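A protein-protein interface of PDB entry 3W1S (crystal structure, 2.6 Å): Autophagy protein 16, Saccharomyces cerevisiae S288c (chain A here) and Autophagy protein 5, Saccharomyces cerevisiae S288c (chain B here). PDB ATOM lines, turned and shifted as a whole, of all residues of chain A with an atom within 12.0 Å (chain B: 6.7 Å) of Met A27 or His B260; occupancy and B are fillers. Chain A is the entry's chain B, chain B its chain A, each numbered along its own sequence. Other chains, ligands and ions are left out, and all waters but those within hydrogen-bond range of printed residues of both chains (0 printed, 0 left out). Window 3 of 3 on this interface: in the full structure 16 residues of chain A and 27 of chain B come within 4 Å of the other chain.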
ATOM      1  N   ASP A  25      -6.416  16.705 -10.963  1.00  0.00           N
ATOM      2  CA  ASP A  25      -5.057  16.089 -10.894  1.00  0.00           C
ATOM      3  C   ASP A  25      -4.243  16.698  -9.752  1.00  0.00           C
ATOM      4  O   ASP A  25      -3.788  15.986  -8.854  1.00  0.00           O
ATOM      5  CB  ASP A  25      -4.323  16.283 -12.227  1.00  0.00           C
ATOM      6  N   SER A  26      -4.059  18.016  -9.790  1.00  0.00           N
ATOM      7  CA  SER A  26      -3.303  18.705  -8.753  1.00  0.00           C
ATOM      8  C   SER A  26      -4.172  19.756  -8.068  1.00  0.00           C
ATOM      9  O   SER A  26      -3.988  20.051  -6.882  1.00  0.00           O
ATOM     10  CB  SER A  26      -2.057  19.363  -9.348  1.00  0.00           C
ATOM     11  OG  SER A  26      -1.203  19.850  -8.325  1.00  0.00           O
ATOM     12  N   MET A  27      -5.114  20.327  -8.819  1.00  0.00           N
ATOM     13  CA  MET A  27      -6.027  21.321  -8.262  1.00  0.00           C
ATOM     14  C   MET A  27      -6.969  20.575  -7.318  1.00  0.00           C
ATOM     15  O   MET A  27      -7.390  21.103  -6.289  1.00  0.00           O
ATOM     16  CB  MET A  27      -6.827  22.002  -9.375  1.00  0.00           C
ATOM     17  CG  MET A  27      -7.849  23.030  -8.882  1.00  0.00           C
ATOM     18  SD  MET A  27      -7.132  24.412  -7.930  1.00  0.00           S
ATOM     19  CE  MET A  27      -7.062  25.699  -9.163  1.00  0.00           C
ATOM     20  N   ASP A  28      -7.280  19.334  -7.682  1.00  0.00           N
ATOM     21  CA  ASP A  28      -8.146  18.480  -6.885  1.00  0.00           C
ATOM     22  C   ASP A  28      -7.476  18.147  -5.561  1.00  0.00           C
ATOM     23  O   ASP A  28      -8.138  18.050  -4.521  1.00  0.00           O
ATOM     24  CB  ASP A  28      -8.446  17.189  -7.642  1.00  0.00           C
ATOM     25  CG  ASP A  28      -9.627  17.326  -8.575  1.00  0.00           C
ATOM     26  OD1 ASP A  28      -9.950  18.469  -8.960  1.00  0.00           O
ATOM     27  OD2 ASP A  28     -10.233  16.291  -8.930  1.00  0.00           O
ATOM     28  N   ASP A  29      -6.157  17.962  -5.610  1.00  0.00           N
ATOM     29  CA  ASP A  29      -5.382  17.647  -4.419  1.00  0.00           C
ATOM     30  C   ASP A  29      -5.423  18.823  -3.457  1.00  0.00           C
ATOM     31  O   ASP A  29      -5.519  18.638  -2.245  1.00  0.00           O
ATOM     32  CB  ASP A  29      -3.931  17.328  -4.788  1.00  0.00           C
ATOM     33  CG  ASP A  29      -3.793  16.038  -5.583  1.00  0.00           C
ATOM     34  OD1 ASP A  29      -4.520  15.065  -5.281  1.00  0.00           O
ATOM     35  OD2 ASP A  29      -2.941  15.988  -6.496  1.00  0.00           O
ATOM     36  N   LEU A  30      -5.353  20.032  -4.003  1.00  0.00           N
ATOM     37  CA  LEU A  30      -5.393  21.244  -3.193  1.00  0.00           C
ATOM     38  C   LEU A  30      -6.795  21.427  -2.612  1.00  0.00           C
ATOM     39  O   LEU A  30      -6.956  21.915  -1.489  1.00  0.00           O
ATOM     40  CB  LEU A  30      -5.001  22.457  -4.043  1.00  0.00           C
ATOM     41  CG  LEU A  30      -5.079  23.853  -3.416  1.00  0.00           C
ATOM     42  CD1 LEU A  30      -4.164  24.779  -4.178  1.00  0.00           C
ATOM     43  CD2 LEU A  30      -6.508  24.385  -3.439  1.00  0.00           C
ATOM     44  N   LEU A  31      -7.802  21.032  -3.389  1.00  0.00           N
ATOM     45  CA  LEU A  31      -9.197  21.115  -2.970  1.00  0.00           C
ATOM     46  C   LEU A  31      -9.383  20.100  -1.851  1.00  0.00           C
ATOM     47  O   LEU A  31      -9.825  20.430  -0.753  1.00  0.00           O
ATOM     48  CB  LEU A  31     -10.114  20.767  -4.147  1.00  0.00           C
ATOM     49  CG  LEU A  31     -11.104  21.793  -4.715  1.00  0.00           C
ATOM     50  CD1 LEU A  31     -10.489  23.177  -4.803  1.00  0.00           C
ATOM     51  CD2 LEU A  31     -11.545  21.318  -6.090  1.00  0.00           C
ATOM     52  N   ILE A  32      -9.024  18.859  -2.143  1.00  0.00           N
ATOM     53  CA  ILE A  32      -9.129  17.781  -1.175  1.00  0.00           C
ATOM     54  C   ILE A  32      -8.392  18.073   0.127  1.00  0.00           C
ATOM     55  O   ILE A  32      -8.834  17.676   1.206  1.00  0.00           O
ATOM     56  CB  ILE A  32      -8.582  16.466  -1.761  1.00  0.00           C
ATOM     57  CG1 ILE A  32      -9.591  15.893  -2.761  1.00  0.00           C
ATOM     58  CG2 ILE A  32      -8.273  15.484  -0.641  1.00  0.00           C
ATOM     59  CD1 ILE A  32      -9.213  14.544  -3.327  1.00  0.00           C
ATOM     60  N   ARG A  33      -7.272  18.769   0.035  1.00  0.00           N
ATOM     61  CA  ARG A  33      -6.504  19.064   1.229  1.00  0.00           C
ATOM     62  C   ARG A  33      -7.097  20.203   2.050  1.00  0.00           C
ATOM     63  O   ARG A  33      -7.131  20.130   3.280  1.00  0.00           O
ATOM     64  CB  ARG A  33      -5.058  19.388   0.857  1.00  0.00           C
ATOM     65  CG  ARG A  33      -4.104  19.438   2.045  1.00  0.00           C
ATOM     66  CD  ARG A  33      -2.780  20.020   1.614  1.00  0.00           C
ATOM     67  NE  ARG A  33      -2.958  21.393   1.160  1.00  0.00           N
ATOM     68  CZ  ARG A  33      -2.370  21.909   0.085  1.00  0.00           C
ATOM     69  NH1 ARG A  33      -2.596  23.176  -0.247  1.00  0.00           N
ATOM     70  NH2 ARG A  33      -1.569  21.155  -0.659  1.00  0.00           N
ATOM     71  N   ARG A  34      -7.557  21.258   1.384  1.00  0.00           N
ATOM     72  CA  ARG A  34      -8.144  22.386   2.103  1.00  0.00           C
ATOM     73  C   ARG A  34      -9.455  21.995   2.793  1.00  0.00           C
ATOM     74  O   ARG A  34      -9.728  22.414   3.917  1.00  0.00           O
ATOM     75  CB  ARG A  34      -8.371  23.559   1.154  1.00  0.00           C
ATOM     76  CG  ARG A  34      -7.089  24.049   0.563  1.00  0.00           C
ATOM     77  CD  ARG A  34      -7.223  25.400  -0.061  1.00  0.00           C
ATOM     78  NE  ARG A  34      -5.959  25.750  -0.684  1.00  0.00           N
ATOM     79  CZ  ARG A  34      -5.722  26.887  -1.313  1.00  0.00           C
ATOM     80  NH1 ARG A  34      -6.670  27.805  -1.411  1.00  0.00           N
ATOM     81  NH2 ARG A  34      -4.529  27.104  -1.838  1.00  0.00           N
ATOM     82  N   LEU A  35     -10.253  21.176   2.117  1.00  0.00           N
ATOM     83  CA  LEU A  35     -11.513  20.719   2.674  1.00  0.00           C
ATOM     84  C   LEU A  35     -11.257  19.781   3.862  1.00  0.00           C
ATOM     85  O   LEU A  35     -11.966  19.836   4.871  1.00  0.00           O
ATOM     86  CB  LEU A  35     -12.342  20.033   1.578  1.00  0.00           C
ATOM     87  CG  LEU A  35     -12.774  20.986   0.443  1.00  0.00           C
ATOM     88  CD1 LEU A  35     -13.507  20.213  -0.639  1.00  0.00           C
ATOM     89  CD2 LEU A  35     -13.658  22.089   0.995  1.00  0.00           C
ATOM     90  N   THR A  36     -10.236  18.934   3.744  1.00  0.00           N
ATOM     91  CA  THR A  36      -9.882  18.004   4.814  1.00  0.00           C
ATOM     92  C   THR A  36      -9.511  18.789   6.064  1.00  0.00           C
ATOM     93  O   THR A  36      -9.842  18.390   7.175  1.00  0.00           O
ATOM     94  CB  THR A  36      -8.691  17.107   4.409  1.00  0.00           C
ATOM     95  OG1 THR A  36      -9.092  16.228   3.351  1.00  0.00           O
ATOM     96  CG2 THR A  36      -8.235  16.270   5.578  1.00  0.00           C
ATOM     97  N   ASP A  37      -8.824  19.911   5.874  1.00  0.00           N
ATOM     98  CA  ASP A  37      -8.427  20.770   6.986  1.00  0.00           C
ATOM     99  C   ASP A  37      -9.682  21.403   7.548  1.00  0.00           C
ATOM    100  O   ASP A  37      -9.855  21.505   8.764  1.00  0.00           O
ATOM    101  CB  ASP A  37      -7.484  21.899   6.530  1.00  0.00           C
ATOM    102  CG  ASP A  37      -6.105  21.403   6.109  1.00  0.00           C
ATOM    103  OD1 ASP A  37      -5.593  20.417   6.694  1.00  0.00           O
ATOM    104  OD2 ASP A  37      -5.521  22.027   5.194  1.00  0.00           O
ATOM    105  N   ILE B   4     -13.817  14.458  -3.206  1.00  0.00           N
ATOM    106  CA  ILE B   4     -14.187  15.825  -2.862  1.00  0.00           C
ATOM    107  C   ILE B   4     -15.613  15.936  -2.324  1.00  0.00           C
ATOM    108  O   ILE B   4     -15.832  16.435  -1.217  1.00  0.00           O
ATOM    109  CB  ILE B   4     -14.032  16.745  -4.094  1.00  0.00           C
ATOM    110  CG1 ILE B   4     -12.554  16.833  -4.479  1.00  0.00           C
ATOM    111  CG2 ILE B   4     -14.623  18.115  -3.810  1.00  0.00           C
ATOM    112  CD1 ILE B   4     -12.270  17.613  -5.743  1.00  0.00           C
ATOM    113  N   THR B 228     -12.365  31.437 -16.085  1.00  0.00           N
ATOM    114  CA  THR B 228     -11.812  31.185 -14.764  1.00  0.00           C
ATOM    115  C   THR B 228     -12.459  32.266 -13.918  1.00  0.00           C
ATOM    116  O   THR B 228     -13.116  33.164 -14.460  1.00  0.00           O
ATOM    117  CB  THR B 228     -10.281  31.388 -14.733  1.00  0.00           C
ATOM    118  OG1 THR B 228      -9.974  32.732 -15.128  1.00  0.00           O
ATOM    119  CG2 THR B 228      -9.586  30.402 -15.673  1.00  0.00           C
ATOM    120  N   LEU B 229     -12.289  32.191 -12.604  1.00  0.00           N
ATOM    121  CA  LEU B 229     -12.885  33.204 -11.754  1.00  0.00           C
ATOM    122  C   LEU B 229     -12.386  34.570 -12.213  1.00  0.00           C
ATOM    123  O   LEU B 229     -13.154  35.537 -12.257  1.00  0.00           O
ATOM    124  CB  LEU B 229     -12.524  32.968 -10.284  1.00  0.00           C
ATOM    125  CG  LEU B 229     -13.016  31.659  -9.660  1.00  0.00           C
ATOM    126  CD1 LEU B 229     -12.683  31.650  -8.171  1.00  0.00           C
ATOM    127  CD2 LEU B 229     -14.510  31.514  -9.872  1.00  0.00           C
ATOM    128  N   LYS B 230     -11.103  34.640 -12.571  1.00  0.00           N
ATOM    129  CA  LYS B 230     -10.506  35.889 -13.029  1.00  0.00           C
ATOM    130  C   LYS B 230     -11.251  36.388 -14.253  1.00  0.00           C
ATOM    131  O   LYS B 230     -11.623  37.560 -14.329  1.00  0.00           O
ATOM    132  CB  LYS B 230      -9.027  35.687 -13.359  1.00  0.00           C
ATOM    133  N   ILE B 257     -10.265  29.869  -2.649  1.00  0.00           N
ATOM    134  CA  ILE B 257     -10.234  29.388  -4.022  1.00  0.00           C
ATOM    135  C   ILE B 257      -9.290  30.232  -4.882  1.00  0.00           C
ATOM    136  O   ILE B 257      -9.327  31.465  -4.854  1.00  0.00           O
ATOM    137  CB  ILE B 257     -11.645  29.396  -4.652  1.00  0.00           C
ATOM    138  CG1 ILE B 257     -12.607  28.576  -3.787  1.00  0.00           C
ATOM    139  CG2 ILE B 257     -11.595  28.815  -6.060  1.00  0.00           C
ATOM    140  CD1 ILE B 257     -12.224  27.111  -3.631  1.00  0.00           C
ATOM    141  N   PRO B 258      -8.409  29.568  -5.637  1.00  0.00           N
ATOM    142  CA  PRO B 258      -7.462  30.273  -6.502  1.00  0.00           C
ATOM    143  C   PRO B 258      -8.215  30.956  -7.640  1.00  0.00           C
ATOM    144  O   PRO B 258      -9.074  30.335  -8.261  1.00  0.00           O
ATOM    145  CB  PRO B 258      -6.560  29.147  -7.011  1.00  0.00           C
ATOM    146  CG  PRO B 258      -6.616  28.137  -5.893  1.00  0.00           C
ATOM    147  CD  PRO B 258      -8.080  28.135  -5.556  1.00  0.00           C
ATOM    148  N   TRP B 259      -7.900  32.219  -7.912  1.00  0.00           N
ATOM    149  CA  TRP B 259      -8.573  32.930  -8.990  1.00  0.00           C
ATOM    150  C   TRP B 259      -8.308  32.322 -10.360  1.00  0.00           C
ATOM    151  O   TRP B 259      -8.994  32.657 -11.315  1.00  0.00           O
ATOM    152  CB  TRP B 259      -8.162  34.401  -9.041  1.00  0.00           C
ATOM    153  CG  TRP B 259      -8.750  35.263  -7.971  1.00  0.00           C
ATOM    154  CD1 TRP B 259      -8.265  35.451  -6.710  1.00  0.00           C
ATOM    155  CD2 TRP B 259      -9.931  36.072  -8.073  1.00  0.00           C
ATOM    156  NE1 TRP B 259      -9.068  36.331  -6.018  1.00  0.00           N
ATOM    157  CE2 TRP B 259     -10.098  36.727  -6.832  1.00  0.00           C
ATOM    158  CE3 TRP B 259     -10.864  36.309  -9.094  1.00  0.00           C
ATOM    159  CZ2 TRP B 259     -11.164  37.606  -6.581  1.00  0.00           C
ATOM    160  CZ3 TRP B 259     -11.927  37.184  -8.843  1.00  0.00           C
ATOM    161  CH2 TRP B 259     -12.064  37.821  -7.596  1.00  0.00           C
ATOM    162  N   HIS B 260      -7.316  31.447 -10.472  1.00  0.00           N
ATOM    163  CA  HIS B 260      -7.017  30.846 -11.768  1.00  0.00           C
ATOM    164  C   HIS B 260      -7.774  29.547 -11.965  1.00  0.00           C
ATOM    165  O   HIS B 260      -7.514  28.801 -12.906  1.00  0.00           O
ATOM    166  CB  HIS B 260      -5.513  30.591 -11.928  1.00  0.00           C
ATOM    167  CG  HIS B 260      -4.959  29.574 -10.980  1.00  0.00           C
ATOM    168  ND1 HIS B 260      -4.608  29.875  -9.680  1.00  0.00           N
ATOM    169  CD2 HIS B 260      -4.679  28.259 -11.148  1.00  0.00           C
ATOM    170  CE1 HIS B 260      -4.132  28.791  -9.090  1.00  0.00           C
ATOM    171  NE2 HIS B 260      -4.165  27.796  -9.959  1.00  0.00           N
ATOM    172  N   MET B 261      -8.715  29.286 -11.068  1.00  0.00           N
ATOM    173  CA  MET B 261      -9.519  28.077 -11.143  1.00  0.00           C
ATOM    174  C   MET B 261     -10.641  28.213 -12.175  1.00  0.00           C
ATOM    175  O   MET B 261     -11.222  29.286 -12.344  1.00  0.00           O
ATOM    176  CB  MET B 261     -10.082  27.739  -9.756  1.00  0.00           C
ATOM    177  CG  MET B 261     -11.277  26.812  -9.776  1.00  0.00           C
ATOM    178  SD  MET B 261     -11.326  25.694  -8.384  1.00  0.00           S
ATOM    179  CE  MET B 261     -11.172  24.161  -9.253  1.00  0.00           C
ATOM    180  N   LEU B 262     -10.916  27.117 -12.877  1.00  0.00           N
ATOM    181  CA  LEU B 262     -11.955  27.080 -13.898  1.00  0.00           C
ATOM    182  C   LEU B 262     -13.344  27.119 -13.266  1.00  0.00           C
ATOM    183  O   LEU B 262     -13.659  26.312 -12.398  1.00  0.00           O
ATOM    184  CB  LEU B 262     -11.806  25.810 -14.740  1.00  0.00           C
ATOM    185  CG  LEU B 262     -10.456  25.653 -15.460  1.00  0.00           C
ATOM    186  CD1 LEU B 262     -10.433  24.342 -16.246  1.00  0.00           C
ATOM    187  CD2 LEU B 262     -10.223  26.836 -16.394  1.00  0.00           C
ATOM    188  N   ASP B 265     -15.201  23.755 -13.317  1.00  0.00           N
ATOM    189  CA  ASP B 265     -14.743  22.758 -12.338  1.00  0.00           C
ATOM    190  C   ASP B 265     -15.195  23.109 -10.934  1.00  0.00           C
ATOM    191  O   ASP B 265     -15.574  22.231 -10.168  1.00  0.00           O
ATOM    192  CB  ASP B 265     -13.222  22.640 -12.306  1.00  0.00           C
ATOM    193  CG  ASP B 265     -12.657  22.062 -13.560  1.00  0.00           C
ATOM    194  OD1 ASP B 265     -13.300  21.169 -14.147  1.00  0.00           O
ATOM    195  OD2 ASP B 265     -11.553  22.496 -13.948  1.00  0.00           O
ATOM    196  N   LYS B 269     -17.764  20.699  -8.916  1.00  0.00           N
ATOM    197  CA  LYS B 269     -17.157  20.053  -7.755  1.00  0.00           C
ATOM    198  C   LYS B 269     -17.612  20.584  -6.402  1.00  0.00           C
ATOM    199  O   LYS B 269     -17.871  19.805  -5.499  1.00  0.00           O
ATOM    200  CB  LYS B 269     -15.619  20.126  -7.844  1.00  0.00           C
ATOM    201  CG  LYS B 269     -15.030  19.089  -8.793  1.00  0.00           C
ATOM    202  CD  LYS B 269     -13.606  19.413  -9.277  1.00  0.00           C
ATOM    203  CE  LYS B 269     -13.108  18.261 -10.150  1.00  0.00           C
ATOM    204  NZ  LYS B 269     -11.828  18.551 -10.829  1.00  0.00           N
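Among the printed residues, merely in contact across the chains: Met A27 with His B260 (3.7 Å), Met A27 with Met B261 (3.5 Å), Asp A28 with Ile B4 (3.9 Å), Leu A31 with Ile B4 (3.8 Å), Ile A32 with Ile B4 (3.6 Å) and Leu A35 with Ile B4 (3.96 Å).
Hydrophobic or aromatic side chains of chain A that line the printed part of chain B: Met A27, Leu A31, Ile A32 and Leu A35. Of the 12 printed residues of chain B, 4 touch a printed residue of chain A. Hydrophobic or aromatic side chains of chain B that line the printed part of chain A: Ile B4, His B260 and Met B261. Among the printed residues, 7 pairs touch across the chains.
The side-chain amino group of Lys B269 is in salt-bridge range of the side-chain carboxylate of Asp A28.
The side-chain hydroxyl (OG1) of Thr A36 sits at hydrogen-bond distance from the backbone carbonyl oxygen (O) of Ile A32, at 2.6 Å. O of Met B261 lies within hydrogen-bond range of N of Leu B229, at 3.1 Å.
Asp A25 touches none of the printed residues of chain B. Met A27 touches two residues of chain B. Printed residues of chain B within 4 Å of Asp A28: Ile B4 (3.9 Å) and Lys B269 (2.7 Å). Leu A30 touches none of the printed residues of chain B. Printed residues of chain B within 4 Å of Leu A31: Ile B4 (3.8 Å). Printed residues of chain B within 4 Å of Ile A32: Ile B4 (3.6 Å). No residue of chain A comes within 4 Å of Thr B228. No residue of chain A comes within 4 Å of Leu B229. Pro B258 touches none of the printed residues of chain A. Of the printed residues of chain A, His B260 touches Met A27. Met B261 touches just one residue of chain A: Met A27 (3.5 Å). Printed residues of chain A within 4 Å of Lys B269: Asp A28. The nearest residue of chain A that does not touch His B260 is Leu A30 (6.3 Å). The nearest printed residue of chain A that does not touch Lys B269 is Leu A31 (4.2 Å).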
